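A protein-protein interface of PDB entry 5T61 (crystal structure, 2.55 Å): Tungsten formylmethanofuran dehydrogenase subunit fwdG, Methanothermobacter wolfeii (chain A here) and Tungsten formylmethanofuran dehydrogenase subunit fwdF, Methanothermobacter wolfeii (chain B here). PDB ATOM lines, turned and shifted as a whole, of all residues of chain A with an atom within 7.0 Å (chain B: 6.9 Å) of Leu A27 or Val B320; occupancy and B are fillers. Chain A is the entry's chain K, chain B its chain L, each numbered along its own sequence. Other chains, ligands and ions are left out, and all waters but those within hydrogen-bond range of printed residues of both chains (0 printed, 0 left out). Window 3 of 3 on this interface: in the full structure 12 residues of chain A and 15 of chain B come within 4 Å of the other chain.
Hydrophobic or aromatic side chains of chain B within 4 Å of the printed part of chain A: Pro B319 and Val B320. Along chain B the printed residues that touch a printed residue of chain A span positions 272 to 320. Of the 13 printed residues of chain A, 4 touch a printed residue of chain B. Among the printed residues, 8 pairs touch across the chains.
Gln B272 touches Pro A23 (CG to O, 3.3 Å). Pro A23 touches Pro B319. Pro A23 touches Val B320 (O to CG1, 3.9 Å). Val A24 touches Pro B319 (CG2 to O, 3.7 Å). Val A24 touches Val B320 (CA to CG1, 3.9 Å). Ala A26 touches Gln B272 (CB to OE1, 3.5 Å). Gln B272 touches Leu A27. CD2 of Leu A27 touches CG1 of Val B320, 3.8 Å away.
Of the printed residues of chain B, Leu A27 touches Gln B272 and Val B320. Of chain A, only Pro A23 (3.9 Å), Val A24 (3.9 Å) and Leu A27 (3.8 Å) come within 4 Å of Val B320. Printed residues of chain B within 4 Å of Val A24: Pro B319 and Val B320. Printed residues of chain B within 4 Å of Pro A23: Gln B272, Pro B319 and Val B320. Printed residues of chain B within 4 Å of Ala A26: Gln B272 (3.5 Å).
NE2 of Gln B272 is in hydrogen-bond range of O of Asp B269 (3.3 Å). SG of Cys B318 sits close to N of Val B320, 3.2 Å away. N of Val A24 sits close to SG of Cys A22 (3.3 Å). The backbone carbonyl oxygen (O) of Thr B270 lies within hydrogen-bond range of the side-chain amide nitrogen (NE2) of Gln B272 (3.0 Å).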
ATOM      1  N   CYS A  22      25.174  -2.239 -13.026  1.00  0.00           N
ATOM      2  CA  CYS A  22      25.447  -3.502 -13.702  1.00  0.00           C
ATOM      3  C   CYS A  22      24.412  -4.572 -13.381  1.00  0.00           C
ATOM      4  O   CYS A  22      24.246  -4.928 -12.204  1.00  0.00           O
ATOM      5  CB  CYS A  22      26.820  -4.005 -13.281  1.00  0.00           C
ATOM      6  SG  CYS A  22      27.003  -5.793 -13.466  1.00  0.00           S
ATOM      7  N   PRO A  23      23.748  -5.154 -14.385  1.00  0.00           N
ATOM      8  CA  PRO A  23      22.737  -6.183 -14.091  1.00  0.00           C
ATOM      9  C   PRO A  23      23.329  -7.481 -13.578  1.00  0.00           C
ATOM     10  O   PRO A  23      22.687  -8.155 -12.764  1.00  0.00           O
ATOM     11  CB  PRO A  23      22.023  -6.380 -15.435  1.00  0.00           C
ATOM     12  CG  PRO A  23      22.948  -5.849 -16.459  1.00  0.00           C
ATOM     13  CD  PRO A  23      23.843  -4.840 -15.820  1.00  0.00           C
ATOM     14  N   VAL A  24      24.524  -7.864 -14.035  1.00  0.00           N
ATOM     15  CA  VAL A  24      25.158  -9.067 -13.500  1.00  0.00           C
ATOM     16  C   VAL A  24      25.389  -8.908 -12.004  1.00  0.00           C
ATOM     17  O   VAL A  24      25.047  -9.789 -11.210  1.00  0.00           O
ATOM     18  CB  VAL A  24      26.469  -9.374 -14.245  1.00  0.00           C
ATOM     19  CG1 VAL A  24      27.173 -10.568 -13.601  1.00  0.00           C
ATOM     20  CG2 VAL A  24      26.203  -9.634 -15.716  1.00  0.00           C
ATOM     21  N   ASN A  25      25.957  -7.768 -11.597  1.00  0.00           N
ATOM     22  CA  ASN A  25      26.138  -7.502 -10.173  1.00  0.00           C
ATOM     23  C   ASN A  25      24.801  -7.501  -9.440  1.00  0.00           C
ATOM     24  O   ASN A  25      24.670  -8.094  -8.362  1.00  0.00           O
ATOM     25  CB  ASN A  25      26.856  -6.166  -9.955  1.00  0.00           C
ATOM     26  CG  ASN A  25      28.254  -6.134 -10.554  1.00  0.00           C
ATOM     27  OD1 ASN A  25      28.792  -7.159 -10.972  1.00  0.00           O
ATOM     28  ND2 ASN A  25      28.856  -4.951 -10.574  1.00  0.00           N
ATOM     29  N   ALA A  26      23.799  -6.819 -10.004  1.00  0.00           N
ATOM     30  CA  ALA A  26      22.489  -6.738  -9.362  1.00  0.00           C
ATOM     31  C   ALA A  26      21.898  -8.127  -9.139  1.00  0.00           C
ATOM     32  O   ALA A  26      21.435  -8.446  -8.033  1.00  0.00           O
ATOM     33  CB  ALA A  26      21.544  -5.883 -10.216  1.00  0.00           C
ATOM     34  N   LEU A  27      21.913  -8.971 -10.179  1.00  0.00           N
ATOM     35  CA  LEU A  27      21.356 -10.312 -10.063  1.00  0.00           C
ATOM     36  C   LEU A  27      22.091 -11.113  -9.001  1.00  0.00           C
ATOM     37  O   LEU A  27      21.489 -11.965  -8.336  1.00  0.00           O
ATOM     38  CB  LEU A  27      21.415 -11.048 -11.415  1.00  0.00           C
ATOM     39  CG  LEU A  27      21.097 -12.552 -11.434  1.00  0.00           C
ATOM     40  CD1 LEU A  27      19.630 -12.811 -11.102  1.00  0.00           C
ATOM     41  CD2 LEU A  27      21.474 -13.153 -12.783  1.00  0.00           C
ATOM     42  N   ARG A  28      23.388 -10.861  -8.837  1.00  0.00           N
ATOM     43  CA  ARG A  28      24.204 -11.676  -7.952  1.00  0.00           C
ATOM     44  C   ARG A  28      24.187 -11.213  -6.503  1.00  0.00           C
ATOM     45  O   ARG A  28      24.430 -12.030  -5.609  1.00  0.00           O
ATOM     46  CB  ARG A  28      25.649 -11.678  -8.447  1.00  0.00           C
ATOM     47  CG  ARG A  28      25.764 -12.334  -9.784  1.00  0.00           C
ATOM     48  CD  ARG A  28      27.141 -12.826 -10.044  1.00  0.00           C
ATOM     49  NE  ARG A  28      27.037 -13.978 -10.921  1.00  0.00           N
ATOM     50  CZ  ARG A  28      27.892 -14.988 -10.925  1.00  0.00           C
ATOM     51  NH1 ARG A  28      28.915 -14.990 -10.082  1.00  0.00           N
ATOM     52  NH2 ARG A  28      27.716 -15.997 -11.766  1.00  0.00           N
ATOM     53  N   SER A  29      23.920  -9.937  -6.248  1.00  0.00           N
ATOM     54  CA  SER A  29      23.939  -9.402  -4.894  1.00  0.00           C
ATOM     55  C   SER A  29      22.732  -8.502  -4.653  1.00  0.00           C
ATOM     56  O   SER A  29      22.678  -7.388  -5.190  1.00  0.00           O
ATOM     57  CB  SER A  29      25.238  -8.634  -4.647  1.00  0.00           C
ATOM     58  OG  SER A  29      25.198  -7.964  -3.402  1.00  0.00           O
ATOM     59  N   PRO A  30      21.745  -8.944  -3.867  1.00  0.00           N
ATOM     60  CA  PRO A  30      20.608  -8.055  -3.562  1.00  0.00           C
ATOM     61  C   PRO A  30      21.009  -6.729  -2.934  1.00  0.00           C
ATOM     62  O   PRO A  30      20.310  -5.728  -3.137  1.00  0.00           O
ATOM     63  CB  PRO A  30      19.742  -8.894  -2.614  1.00  0.00           C
ATOM     64  CG  PRO A  30      20.131 -10.301  -2.858  1.00  0.00           C
ATOM     65  CD  PRO A  30      21.544 -10.314  -3.365  1.00  0.00           C
ATOM     66  N   VAL A  32      23.726  -5.010  -3.719  1.00  0.00           N
ATOM     67  CA  VAL A  32      24.147  -4.194  -4.856  1.00  0.00           C
ATOM     68  C   VAL A  32      22.944  -3.779  -5.693  1.00  0.00           C
ATOM     69  O   VAL A  32      22.855  -2.631  -6.143  1.00  0.00           O
ATOM     70  CB  VAL A  32      25.199  -4.944  -5.695  1.00  0.00           C
ATOM     71  CG1 VAL A  32      25.411  -4.245  -7.031  1.00  0.00           C
ATOM     72  CG2 VAL A  32      26.510  -5.025  -4.938  1.00  0.00           C
ATOM     73  N   ALA A  33      22.005  -4.704  -5.922  1.00  0.00           N
ATOM     74  CA  ALA A  33      20.782  -4.357  -6.640  1.00  0.00           C
ATOM     75  C   ALA A  33      20.057  -3.202  -5.961  1.00  0.00           C
ATOM     76  O   ALA A  33      19.463  -2.349  -6.631  1.00  0.00           O
ATOM     77  CB  ALA A  33      19.872  -5.579  -6.752  1.00  0.00           C
ATOM     78  N   LEU A  60      32.556 -12.578 -16.455  1.00  0.00           N
ATOM     79  CA  LEU A  60      31.098 -12.498 -16.383  1.00  0.00           C
ATOM     80  C   LEU A  60      30.537 -11.271 -17.087  1.00  0.00           C
ATOM     81  O   LEU A  60      29.312 -11.149 -17.202  1.00  0.00           O
ATOM     82  CB  LEU A  60      30.606 -12.531 -14.933  1.00  0.00           C
ATOM     83  CG  LEU A  60      30.768 -13.863 -14.208  1.00  0.00           C
ATOM     84  CD1 LEU A  60      30.551 -13.706 -12.719  1.00  0.00           C
ATOM     85  CD2 LEU A  60      29.734 -14.815 -14.784  1.00  0.00           C
ATOM     86  N   GLY A  62      29.187  -9.100 -19.895  1.00  0.00           N
ATOM     87  CA  GLY A  62      28.582  -9.288 -21.197  1.00  0.00           C
ATOM     88  C   GLY A  62      28.690  -8.095 -22.122  1.00  0.00           C
ATOM     89  O   GLY A  62      28.079  -8.109 -23.195  1.00  0.00           O
ATOM     90  N   ASP B 269      12.356 -12.258 -13.184  1.00  0.00           N
ATOM     91  CA  ASP B 269      13.175 -12.181 -11.978  1.00  0.00           C
ATOM     92  C   ASP B 269      14.665 -12.154 -12.293  1.00  0.00           C
ATOM     93  O   ASP B 269      15.436 -11.522 -11.563  1.00  0.00           O
ATOM     94  CB  ASP B 269      12.876 -13.356 -11.046  1.00  0.00           C
ATOM     95  CG  ASP B 269      11.465 -13.324 -10.496  1.00  0.00           C
ATOM     96  OD1 ASP B 269      11.066 -12.277  -9.945  1.00  0.00           O
ATOM     97  OD2 ASP B 269      10.759 -14.349 -10.606  1.00  0.00           O
ATOM     98  N   THR B 270      15.090 -12.817 -13.369  1.00  0.00           N
ATOM     99  CA  THR B 270      16.483 -12.712 -13.790  1.00  0.00           C
ATOM    100  C   THR B 270      16.786 -11.313 -14.315  1.00  0.00           C
ATOM    101  O   THR B 270      17.881 -10.781 -14.094  1.00  0.00           O
ATOM    102  CB  THR B 270      16.784 -13.772 -14.849  1.00  0.00           C
ATOM    103  OG1 THR B 270      16.328 -15.047 -14.382  1.00  0.00           O
ATOM    104  CG2 THR B 270      18.278 -13.850 -15.119  1.00  0.00           C
ATOM    105  N   CYS B 271      15.825 -10.717 -15.014  1.00  0.00           N
ATOM    106  CA  CYS B 271      15.951  -9.362 -15.535  1.00  0.00           C
ATOM    107  C   CYS B 271      16.201  -8.348 -14.420  1.00  0.00           C
ATOM    108  O   CYS B 271      15.490  -8.323 -13.409  1.00  0.00           O
ATOM    109  CB  CYS B 271      14.677  -9.018 -16.311  1.00  0.00           C
ATOM    110  SG  CYS B 271      14.358  -7.277 -16.632  1.00  0.00           S
ATOM    111  N   GLN B 272      17.215  -7.505 -14.612  1.00  0.00           N
ATOM    112  CA  GLN B 272      17.546  -6.429 -13.685  1.00  0.00           C
ATOM    113  C   GLN B 272      17.313  -5.057 -14.298  1.00  0.00           C
ATOM    114  O   GLN B 272      17.762  -4.052 -13.737  1.00  0.00           O
ATOM    115  CB  GLN B 272      19.003  -6.552 -13.230  1.00  0.00           C
ATOM    116  CG  GLN B 272      19.368  -7.918 -12.684  1.00  0.00           C
ATOM    117  CD  GLN B 272      18.599  -8.261 -11.430  1.00  0.00           C
ATOM    118  OE1 GLN B 272      18.475  -7.439 -10.519  1.00  0.00           O
ATOM    119  NE2 GLN B 272      18.060  -9.473 -11.380  1.00  0.00           N
ATOM    120  N   SER B 317      22.199  -9.358 -26.549  1.00  0.00           N
ATOM    121  CA  SER B 317      22.684  -8.211 -25.790  1.00  0.00           C
ATOM    122  C   SER B 317      22.575  -8.399 -24.280  1.00  0.00           C
ATOM    123  O   SER B 317      23.287  -7.716 -23.535  1.00  0.00           O
ATOM    124  CB  SER B 317      21.923  -6.943 -26.196  1.00  0.00           C
ATOM    125  OG  SER B 317      20.589  -6.957 -25.711  1.00  0.00           O
ATOM    126  N   CYS B 318      21.732  -9.314 -23.816  1.00  0.00           N
ATOM    127  CA  CYS B 318      21.437  -9.412 -22.391  1.00  0.00           C
ATOM    128  C   CYS B 318      22.572 -10.100 -21.645  1.00  0.00           C
ATOM    129  O   CYS B 318      22.868 -11.267 -21.924  1.00  0.00           O
ATOM    130  CB  CYS B 318      20.149 -10.179 -22.159  1.00  0.00           C
ATOM    131  SG  CYS B 318      20.030 -10.836 -20.480  1.00  0.00           S
ATOM    132  N   PRO B 319      23.218  -9.430 -20.688  1.00  0.00           N
ATOM    133  CA  PRO B 319      24.344 -10.050 -19.980  1.00  0.00           C
ATOM    134  C   PRO B 319      23.944 -11.089 -18.938  1.00  0.00           C
ATOM    135  O   PRO B 319      24.834 -11.760 -18.401  1.00  0.00           O
ATOM    136  CB  PRO B 319      25.037  -8.850 -19.324  1.00  0.00           C
ATOM    137  CG  PRO B 319      23.954  -7.857 -19.128  1.00  0.00           C
ATOM    138  CD  PRO B 319      22.965  -8.048 -20.241  1.00  0.00           C
ATOM    139  N   VAL B 320      22.657 -11.238 -18.616  1.00  0.00           N
ATOM    140  CA  VAL B 320      22.214 -12.272 -17.690  1.00  0.00           C
ATOM    141  C   VAL B 320      21.313 -13.307 -18.364  1.00  0.00           C
ATOM    142  O   VAL B 320      20.703 -14.129 -17.675  1.00  0.00           O
ATOM    143  CB  VAL B 320      21.512 -11.663 -16.459  1.00  0.00           C
ATOM    144  CG1 VAL B 320      22.485 -10.809 -15.661  1.00  0.00           C
ATOM    145  CG2 VAL B 320      20.296 -10.851 -16.881  1.00  0.00           C
ATOM    146  N   THR B 321      21.248 -13.302 -19.693  1.00  0.00           N
ATOM    147  CA  THR B 321      20.365 -14.164 -20.490  1.00  0.00           C
ATOM    148  C   THR B 321      19.000 -14.334 -19.819  1.00  0.00           C
ATOM    149  O   THR B 321      18.500 -15.440 -19.601  1.00  0.00           O
ATOM    150  CB  THR B 321      21.021 -15.515 -20.780  1.00  0.00           C
ATOM    151  OG1 THR B 321      21.339 -16.177 -19.551  1.00  0.00           O
ATOM    152  CG2 THR B 321      22.297 -15.323 -21.598  1.00  0.00           C
ATOM    153  N   ALA B 322      18.388 -13.197 -19.506  1.00  0.00           N
ATOM    154  CA  ALA B 322      17.043 -13.172 -18.953  1.00  0.00           C
ATOM    155  C   ALA B 322      15.991 -13.214 -20.047  1.00  0.00           C
ATOM    156  O   ALA B 322      14.797 -13.340 -19.750  1.00  0.00           O
ATOM    157  CB  ALA B 322      16.843 -11.924 -18.090  1.00  0.00           C
ATOM    158  N   ILE B 323      16.427 -13.123 -21.298  1.00  0.00           N
ATOM    159  CA  ILE B 323      15.559 -13.074 -22.462  1.00  0.00           C
ATOM    160  C   ILE B 323      16.132 -14.031 -23.504  1.00  0.00           C
ATOM    161  O   ILE B 323      17.321 -13.962 -23.834  1.00  0.00           O
ATOM    162  CB  ILE B 323      15.448 -11.626 -22.981  1.00  0.00           C
ATOM    163  CG1 ILE B 323      14.655 -11.525 -24.281  1.00  0.00           C
ATOM    164  CG2 ILE B 323      16.838 -10.996 -23.121  1.00  0.00           C
ATOM    165  CD1 ILE B 323      14.211 -10.104 -24.548  1.00  0.00           C
